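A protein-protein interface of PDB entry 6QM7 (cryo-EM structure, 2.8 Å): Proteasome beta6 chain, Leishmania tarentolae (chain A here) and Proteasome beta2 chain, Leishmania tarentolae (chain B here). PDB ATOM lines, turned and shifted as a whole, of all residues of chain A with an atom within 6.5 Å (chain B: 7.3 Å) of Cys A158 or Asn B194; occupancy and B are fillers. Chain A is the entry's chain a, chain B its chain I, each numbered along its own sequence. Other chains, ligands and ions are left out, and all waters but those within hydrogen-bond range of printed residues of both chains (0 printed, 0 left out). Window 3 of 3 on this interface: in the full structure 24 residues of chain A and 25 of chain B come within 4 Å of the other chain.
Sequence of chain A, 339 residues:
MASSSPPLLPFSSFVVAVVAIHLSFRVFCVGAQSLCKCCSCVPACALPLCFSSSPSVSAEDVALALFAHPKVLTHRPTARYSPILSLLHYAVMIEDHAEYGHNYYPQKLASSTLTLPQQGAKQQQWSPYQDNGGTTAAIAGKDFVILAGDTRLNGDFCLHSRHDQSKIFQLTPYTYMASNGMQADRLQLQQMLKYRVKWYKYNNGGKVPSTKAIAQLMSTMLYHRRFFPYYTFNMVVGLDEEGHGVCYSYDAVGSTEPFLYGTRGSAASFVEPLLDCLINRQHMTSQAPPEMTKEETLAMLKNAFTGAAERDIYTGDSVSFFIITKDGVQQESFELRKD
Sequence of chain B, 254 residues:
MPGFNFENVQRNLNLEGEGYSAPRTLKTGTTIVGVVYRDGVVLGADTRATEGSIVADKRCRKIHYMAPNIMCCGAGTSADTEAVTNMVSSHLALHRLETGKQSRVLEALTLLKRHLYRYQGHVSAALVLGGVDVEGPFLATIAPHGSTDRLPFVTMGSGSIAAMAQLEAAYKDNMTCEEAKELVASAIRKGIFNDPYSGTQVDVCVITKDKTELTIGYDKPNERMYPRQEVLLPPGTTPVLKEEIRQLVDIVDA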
ATOM      1  N   LEU A 153      29.952  20.710  20.146  1.00  0.00           N
ATOM      2  CA  LEU A 153      30.577  21.765  20.967  1.00  0.00           C
ATOM      3  C   LEU A 153      29.560  22.876  21.047  1.00  0.00           C
ATOM      4  O   LEU A 153      29.333  23.499  20.017  1.00  0.00           O
ATOM      5  CB  LEU A 153      31.842  22.243  20.256  1.00  0.00           C
ATOM      6  CG  LEU A 153      32.501  23.503  20.809  1.00  0.00           C
ATOM      7  CD1 LEU A 153      33.155  23.250  22.155  1.00  0.00           C
ATOM      8  CD2 LEU A 153      33.536  24.009  19.823  1.00  0.00           C
ATOM      9  N   ASN A 154      28.926  23.060  22.191  1.00  0.00           N
ATOM     10  CA  ASN A 154      27.824  24.036  22.287  1.00  0.00           C
ATOM     11  C   ASN A 154      28.349  25.227  23.071  1.00  0.00           C
ATOM     12  O   ASN A 154      29.131  25.018  23.984  1.00  0.00           O
ATOM     13  CB  ASN A 154      26.494  23.417  22.735  1.00  0.00           C
ATOM     14  CG  ASN A 154      26.583  22.339  23.786  1.00  0.00           C
ATOM     15  OD1 ASN A 154      26.602  22.646  24.975  1.00  0.00           O
ATOM     16  ND2 ASN A 154      26.564  21.085  23.365  1.00  0.00           N
ATOM     17  N   GLY A 155      28.020  26.434  22.605  1.00  0.00           N
ATOM     18  CA  GLY A 155      28.342  27.713  23.256  1.00  0.00           C
ATOM     19  C   GLY A 155      27.217  28.103  24.181  1.00  0.00           C
ATOM     20  O   GLY A 155      26.532  27.181  24.672  1.00  0.00           O
ATOM     21  N   ASP A 156      27.019  29.404  24.398  1.00  0.00           N
ATOM     22  CA  ASP A 156      25.956  29.942  25.291  1.00  0.00           C
ATOM     23  C   ASP A 156      24.659  30.041  24.483  1.00  0.00           C
ATOM     24  O   ASP A 156      24.561  30.932  23.617  1.00  0.00           O
ATOM     25  CB  ASP A 156      26.369  31.278  25.924  1.00  0.00           C
ATOM     26  CG  ASP A 156      27.464  31.180  26.986  1.00  0.00           C
ATOM     27  OD1 ASP A 156      28.124  30.114  27.080  1.00  0.00           O
ATOM     28  OD2 ASP A 156      27.656  32.179  27.714  1.00  0.00           O
ATOM     29  N   PHE A 157      23.732  29.107  24.720  1.00  0.00           N
ATOM     30  CA  PHE A 157      22.350  29.080  24.170  1.00  0.00           C
ATOM     31  C   PHE A 157      22.347  28.768  22.664  1.00  0.00           C
ATOM     32  O   PHE A 157      21.239  28.573  22.137  1.00  0.00           O
ATOM     33  CB  PHE A 157      21.617  30.389  24.495  1.00  0.00           C
ATOM     34  CG  PHE A 157      20.443  30.259  25.438  1.00  0.00           C
ATOM     35  CD1 PHE A 157      19.183  30.724  25.071  1.00  0.00           C
ATOM     36  CD2 PHE A 157      20.591  29.681  26.694  1.00  0.00           C
ATOM     37  CE1 PHE A 157      18.101  30.612  25.936  1.00  0.00           C
ATOM     38  CE2 PHE A 157      19.508  29.569  27.556  1.00  0.00           C
ATOM     39  CZ  PHE A 157      18.266  30.034  27.176  1.00  0.00           C
ATOM     40  N   CYS A 158      23.503  28.704  21.993  1.00  0.00           N
ATOM     41  CA  CYS A 158      23.639  28.237  20.585  1.00  0.00           C
ATOM     42  C   CYS A 158      24.545  27.004  20.532  1.00  0.00           C
ATOM     43  O   CYS A 158      24.889  26.481  21.610  1.00  0.00           O
ATOM     44  CB  CYS A 158      24.194  29.331  19.682  1.00  0.00           C
ATOM     45  SG  CYS A 158      25.940  29.692  19.974  1.00  0.00           S
ATOM     46  N   LEU A 159      24.877  26.531  19.329  1.00  0.00           N
ATOM     47  CA  LEU A 159      25.912  25.486  19.145  1.00  0.00           C
ATOM     48  C   LEU A 159      26.927  25.958  18.097  1.00  0.00           C
ATOM     49  O   LEU A 159      26.525  26.528  17.080  1.00  0.00           O
ATOM     50  CB  LEU A 159      25.243  24.133  18.847  1.00  0.00           C
ATOM     51  CG  LEU A 159      25.362  23.552  17.436  1.00  0.00           C
ATOM     52  CD1 LEU A 159      25.533  22.051  17.495  1.00  0.00           C
ATOM     53  CD2 LEU A 159      24.147  23.888  16.599  1.00  0.00           C
ATOM     54  N   HIS A 160      28.207  25.759  18.405  1.00  0.00           N
ATOM     55  CA  HIS A 160      29.383  26.249  17.646  1.00  0.00           C
ATOM     56  C   HIS A 160      29.680  25.302  16.488  1.00  0.00           C
ATOM     57  O   HIS A 160      29.867  25.783  15.354  1.00  0.00           O
ATOM     58  CB  HIS A 160      30.614  26.341  18.559  1.00  0.00           C
ATOM     59  CG  HIS A 160      30.573  27.461  19.544  1.00  0.00           C
ATOM     60  ND1 HIS A 160      29.929  28.658  19.280  1.00  0.00           N
ATOM     61  CD2 HIS A 160      31.152  27.593  20.760  1.00  0.00           C
ATOM     62  CE1 HIS A 160      30.082  29.457  20.317  1.00  0.00           C
ATOM     63  NE2 HIS A 160      30.837  28.832  21.235  1.00  0.00           N
ATOM     64  N   ARG A 162      29.200  20.841  15.169  1.00  0.00           N
ATOM     65  CA  ARG A 162      28.747  19.437  15.312  1.00  0.00           C
ATOM     66  C   ARG A 162      29.928  18.481  15.111  1.00  0.00           C
ATOM     67  O   ARG A 162      29.722  17.272  15.289  1.00  0.00           O
ATOM     68  CB  ARG A 162      27.695  19.126  14.248  1.00  0.00           C
ATOM     69  CG  ARG A 162      26.568  20.141  14.146  1.00  0.00           C
ATOM     70  CD  ARG A 162      25.362  19.567  13.422  1.00  0.00           C
ATOM     71  NE  ARG A 162      24.182  19.693  14.265  1.00  0.00           N
ATOM     72  CZ  ARG A 162      23.311  20.692  14.238  1.00  0.00           C
ATOM     73  NH1 ARG A 162      22.296  20.683  15.083  1.00  0.00           N
ATOM     74  NH2 ARG A 162      23.447  21.697  13.386  1.00  0.00           N
ATOM     75  N   TYR A 314      22.459  18.646  25.420  1.00  0.00           N
ATOM     76  CA  TYR A 314      23.838  19.127  25.139  1.00  0.00           C
ATOM     77  C   TYR A 314      24.709  18.026  24.522  1.00  0.00           C
ATOM     78  O   TYR A 314      25.849  18.329  24.134  1.00  0.00           O
ATOM     79  CB  TYR A 314      24.461  19.697  26.414  1.00  0.00           C
ATOM     80  CG  TYR A 314      23.777  20.950  26.905  1.00  0.00           C
ATOM     81  CD1 TYR A 314      23.611  22.044  26.071  1.00  0.00           C
ATOM     82  CD2 TYR A 314      23.270  21.042  28.194  1.00  0.00           C
ATOM     83  CE1 TYR A 314      22.970  23.194  26.498  1.00  0.00           C
ATOM     84  CE2 TYR A 314      22.629  22.189  28.639  1.00  0.00           C
ATOM     85  CZ  TYR A 314      22.481  23.272  27.788  1.00  0.00           C
ATOM     86  OH  TYR A 314      21.845  24.414  28.191  1.00  0.00           O
ATOM     87  N   ASP A 339      19.503  17.124  16.141  1.00  0.00           N
ATOM     88  CA  ASP A 339      18.819  18.200  16.913  1.00  0.00           C
ATOM     89  C   ASP A 339      19.324  18.233  18.366  1.00  0.00           C
ATOM     90  O   ASP A 339      19.413  19.334  18.934  1.00  0.00           O
ATOM     91  CB  ASP A 339      17.293  18.056  16.844  1.00  0.00           C
ATOM     92  CG  ASP A 339      16.660  17.116  17.857  1.00  0.00           C
ATOM     93  OD1 ASP A 339      15.974  17.620  18.756  1.00  0.00           O
ATOM     94  OD2 ASP A 339      16.820  15.896  17.724  1.00  0.00           O
ATOM     95  OXT ASP A 339      19.651  17.213  19.010  1.00  0.00           O
ATOM     96  N   GLY B 159      14.079  29.404  20.768  1.00  0.00           N
ATOM     97  CA  GLY B 159      14.455  29.299  19.349  1.00  0.00           C
ATOM     98  C   GLY B 159      13.825  30.384  18.507  1.00  0.00           C
ATOM     99  O   GLY B 159      13.841  30.233  17.276  1.00  0.00           O
ATOM    100  N   ALA B 162      16.487  32.267  15.933  1.00  0.00           N
ATOM    101  CA  ALA B 162      16.837  31.364  14.812  1.00  0.00           C
ATOM    102  C   ALA B 162      15.663  31.287  13.846  1.00  0.00           C
ATOM    103  O   ALA B 162      15.888  31.505  12.661  1.00  0.00           O
ATOM    104  CB  ALA B 162      17.202  29.998  15.336  1.00  0.00           C
ATOM    105  N   ALA B 163      14.473  30.984  14.361  1.00  0.00           N
ATOM    106  CA  ALA B 163      13.226  30.842  13.575  1.00  0.00           C
ATOM    107  C   ALA B 163      12.931  32.136  12.831  1.00  0.00           C
ATOM    108  O   ALA B 163      12.630  32.077  11.627  1.00  0.00           O
ATOM    109  CB  ALA B 163      12.076  30.497  14.474  1.00  0.00           C
ATOM    110  N   ALA B 187      11.164  27.477   9.546  1.00  0.00           N
ATOM    111  CA  ALA B 187      11.464  28.369  10.683  1.00  0.00           C
ATOM    112  C   ALA B 187      11.605  27.532  11.946  1.00  0.00           C
ATOM    113  O   ALA B 187      12.562  27.746  12.675  1.00  0.00           O
ATOM    114  CB  ALA B 187      10.379  29.405  10.849  1.00  0.00           C
ATOM    115  N   ILE B 188      10.660  26.636  12.209  1.00  0.00           N
ATOM    116  CA  ILE B 188      10.697  25.762  13.413  1.00  0.00           C
ATOM    117  C   ILE B 188      11.972  24.923  13.333  1.00  0.00           C
ATOM    118  O   ILE B 188      12.702  24.881  14.328  1.00  0.00           O
ATOM    119  CB  ILE B 188       9.441  24.886  13.528  1.00  0.00           C
ATOM    120  CG1 ILE B 188       8.175  25.720  13.715  1.00  0.00           C
ATOM    121  CG2 ILE B 188       9.605  23.892  14.661  1.00  0.00           C
ATOM    122  CD1 ILE B 188       8.222  26.600  14.932  1.00  0.00           C
ATOM    123  N   ARG B 189      12.248  24.320  12.182  1.00  0.00           N
ATOM    124  CA  ARG B 189      13.463  23.495  12.004  1.00  0.00           C
ATOM    125  C   ARG B 189      14.695  24.287  12.450  1.00  0.00           C
ATOM    126  O   ARG B 189      15.542  23.685  13.102  1.00  0.00           O
ATOM    127  CB  ARG B 189      13.586  22.969  10.573  1.00  0.00           C
ATOM    128  CG  ARG B 189      12.807  21.684  10.323  1.00  0.00           C
ATOM    129  CD  ARG B 189      13.326  20.928   9.108  1.00  0.00           C
ATOM    130  NE  ARG B 189      13.453  21.805   7.954  1.00  0.00           N
ATOM    131  CZ  ARG B 189      12.449  22.241   7.185  1.00  0.00           C
ATOM    132  NH1 ARG B 189      12.722  23.058   6.179  1.00  0.00           N
ATOM    133  NH2 ARG B 189      11.190  21.883   7.409  1.00  0.00           N
ATOM    134  N   LYS B 190      14.779  25.585  12.165  1.00  0.00           N
ATOM    135  CA  LYS B 190      15.916  26.430  12.622  1.00  0.00           C
ATOM    136  C   LYS B 190      16.042  26.338  14.138  1.00  0.00           C
ATOM    137  O   LYS B 190      17.171  26.198  14.620  1.00  0.00           O
ATOM    138  CB  LYS B 190      15.761  27.916  12.295  1.00  0.00           C
ATOM    139  CG  LYS B 190      15.670  28.260  10.824  1.00  0.00           C
ATOM    140  CD  LYS B 190      16.882  27.861  10.021  1.00  0.00           C
ATOM    141  CE  LYS B 190      16.512  27.324   8.658  1.00  0.00           C
ATOM    142  NZ  LYS B 190      15.885  25.983   8.745  1.00  0.00           N
ATOM    143  N   GLY B 191      14.935  26.492  14.861  1.00  0.00           N
ATOM    144  CA  GLY B 191      14.930  26.328  16.325  1.00  0.00           C
ATOM    145  C   GLY B 191      15.358  24.911  16.685  1.00  0.00           C
ATOM    146  O   GLY B 191      16.343  24.758  17.422  1.00  0.00           O
ATOM    147  N   ILE B 192      14.682  23.907  16.129  1.00  0.00           N
ATOM    148  CA  ILE B 192      14.938  22.477  16.439  1.00  0.00           C
ATOM    149  C   ILE B 192      16.447  22.229  16.454  1.00  0.00           C
ATOM    150  O   ILE B 192      16.964  21.782  17.513  1.00  0.00           O
ATOM    151  CB  ILE B 192      14.211  21.568  15.446  1.00  0.00           C
ATOM    152  CG1 ILE B 192      12.721  21.494  15.786  1.00  0.00           C
ATOM    153  CG2 ILE B 192      14.859  20.198  15.394  1.00  0.00           C
ATOM    154  CD1 ILE B 192      11.873  20.819  14.733  1.00  0.00           C
ATOM    155  N   PHE B 193      17.119  22.554  15.355  1.00  0.00           N
ATOM    156  CA  PHE B 193      18.513  22.146  15.076  1.00  0.00           C
ATOM    157  C   PHE B 193      19.534  23.067  15.739  1.00  0.00           C
ATOM    158  O   PHE B 193      20.632  22.581  16.023  1.00  0.00           O
ATOM    159  CB  PHE B 193      18.752  22.091  13.570  1.00  0.00           C
ATOM    160  CG  PHE B 193      18.066  20.922  12.922  1.00  0.00           C
ATOM    161  CD1 PHE B 193      18.333  19.627  13.345  1.00  0.00           C
ATOM    162  CD2 PHE B 193      17.138  21.105  11.910  1.00  0.00           C
ATOM    163  CE1 PHE B 193      17.688  18.543  12.774  1.00  0.00           C
ATOM    164  CE2 PHE B 193      16.505  20.015  11.330  1.00  0.00           C
ATOM    165  CZ  PHE B 193      16.780  18.739  11.765  1.00  0.00           C
ATOM    166  N   ASN B 194      19.216  24.337  15.957  1.00  0.00           N
ATOM    167  CA  ASN B 194      20.202  25.365  16.387  1.00  0.00           C
ATOM    168  C   ASN B 194      19.951  25.759  17.846  1.00  0.00           C
ATOM    169  O   ASN B 194      20.875  26.324  18.448  1.00  0.00           O
ATOM    170  CB  ASN B 194      20.205  26.534  15.397  1.00  0.00           C
ATOM    171  CG  ASN B 194      20.505  26.071  13.982  1.00  0.00           C
ATOM    172  OD1 ASN B 194      21.607  25.588  13.715  1.00  0.00           O
ATOM    173  ND2 ASN B 194      19.539  26.173  13.080  1.00  0.00           N
ATOM    174  N   ASP B 195      18.773  25.468  18.398  1.00  0.00           N
ATOM    175  CA  ASP B 195      18.426  25.700  19.823  1.00  0.00           C
ATOM    176  C   ASP B 195      18.382  24.346  20.536  1.00  0.00           C
ATOM    177  O   ASP B 195      17.824  23.371  20.016  1.00  0.00           O
ATOM    178  CB  ASP B 195      17.126  26.501  19.929  1.00  0.00           C
ATOM    179  CG  ASP B 195      16.526  26.603  21.320  1.00  0.00           C
ATOM    180  OD1 ASP B 195      17.306  26.710  22.292  1.00  0.00           O
ATOM    181  OD2 ASP B 195      15.271  26.579  21.424  1.00  0.00           O
ATOM    182  N   PRO B 196      19.023  24.221  21.723  1.00  0.00           N
ATOM    183  CA  PRO B 196      18.943  22.990  22.511  1.00  0.00           C
ATOM    184  C   PRO B 196      17.584  22.747  23.190  1.00  0.00           C
ATOM    185  O   PRO B 196      17.237  21.603  23.359  1.00  0.00           O
ATOM    186  CB  PRO B 196      20.064  23.168  23.547  1.00  0.00           C
ATOM    187  CG  PRO B 196      20.160  24.656  23.716  1.00  0.00           C
ATOM    188  CD  PRO B 196      19.948  25.198  22.319  1.00  0.00           C
ATOM    189  N   TYR B 197      16.853  23.797  23.556  1.00  0.00           N
ATOM    190  CA  TYR B 197      15.534  23.677  24.231  1.00  0.00           C
ATOM    191  C   TYR B 197      14.437  23.303  23.234  1.00  0.00           C
ATOM    192  O   TYR B 197      13.399  22.805  23.702  1.00  0.00           O
ATOM    193  CB  TYR B 197      15.220  24.946  25.023  1.00  0.00           C
ATOM    194  CG  TYR B 197      16.127  25.067  26.217  1.00  0.00           C
ATOM    195  CD1 TYR B 197      15.929  24.267  27.331  1.00  0.00           C
ATOM    196  CD2 TYR B 197      17.237  25.898  26.198  1.00  0.00           C
ATOM    197  CE1 TYR B 197      16.783  24.324  28.420  1.00  0.00           C
ATOM    198  CE2 TYR B 197      18.098  25.969  27.282  1.00  0.00           C
ATOM    199  CZ  TYR B 197      17.873  25.177  28.399  1.00  0.00           C
ATOM    200  OH  TYR B 197      18.713  25.223  29.476  1.00  0.00           O
ATOM    201  N   SER B 198      14.644  23.523  21.937  1.00  0.00           N
ATOM    202  CA  SER B 198      13.701  23.141  20.857  1.00  0.00           C
ATOM    203  C   SER B 198      14.170  21.839  20.228  1.00  0.00           C
ATOM    204  O   SER B 198      15.392  21.663  20.089  1.00  0.00           O
ATOM    205  CB  SER B 198      13.602  24.205  19.809  1.00  0.00           C
ATOM    206  OG  SER B 198      13.166  25.442  20.359  1.00  0.00           O
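Of the 15 printed residues of chain B, 5 touch a printed residue of chain A. Hydrophobic or aromatic side chains of chain B that line the printed part of chain A: Ile B192, Phe B193, Pro B196 and Tyr B197. Along chain A the printed residues that touch a printed residue of chain B span positions 157 to 339. Among the printed residues, 8 pairs touch across the chains.
NH1 of Arg A162 lies within hydrogen-bond range of O of Phe B193, at 2.7 Å. The side-chain hydroxyl (OH) of Tyr B197 is in hydrogen-bond range of the side-chain hydroxyl (OH) of Tyr A314.
ND2 of Asn A154 lies within hydrogen-bond range of O of Tyr A314 (2.9 Å). The backbone carbonyl oxygen (O) of Lys B190 is in hydrogen-bond range of the side-chain amide nitrogen (ND2) of Asn B194 (2.8 Å). The backbone NH of Tyr B197 lies within hydrogen-bond range of the side-chain carboxylate of Asp B195 (3.2 Å).
Asn A154 touches none of the printed residues of chain B. Gly A155 touches none of the printed residues of chain B. Of the printed residues of chain B, Cys A158 touches Asn B194 (3.98 Å). Printed residues of chain B within 4 Å of Arg A162: Phe B193. Of the printed residues of chain B, Tyr A314 touches Tyr B197 (3.5 Å). Printed residues of chain B within 4 Å of Asp A339: Ile B192 and Phe B193. Of the printed residues of chain A, Phe B193 touches Leu A159 (3.8 Å), Arg A162 (2.7 Å) and Asp A339 (3.9 Å). Printed residues of chain A within 4 Å of Asn B194: Cys A158. Of the printed residues of chain A, Tyr B197 touches Phe A157 and Tyr A314. The nearest printed residue of chain B that does not touch Cys A158 is Pro B196 (5.0 Å). The nearest printed residue of chain A that does not touch Asn B194 is Leu A159 (4.1 Å).
Phe A157 touches Pro B196 (O to CD, 3.6 Å). CE2 of Tyr B197 touches CE2 of Phe A157, 3.9 Å away. Cys A158 touches Asn B194. Leu A159 touches Phe B193. Asp A339 touches Ile B192. CD1 of Phe B193 touches CA of Asp A339, 3.9 Å away.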
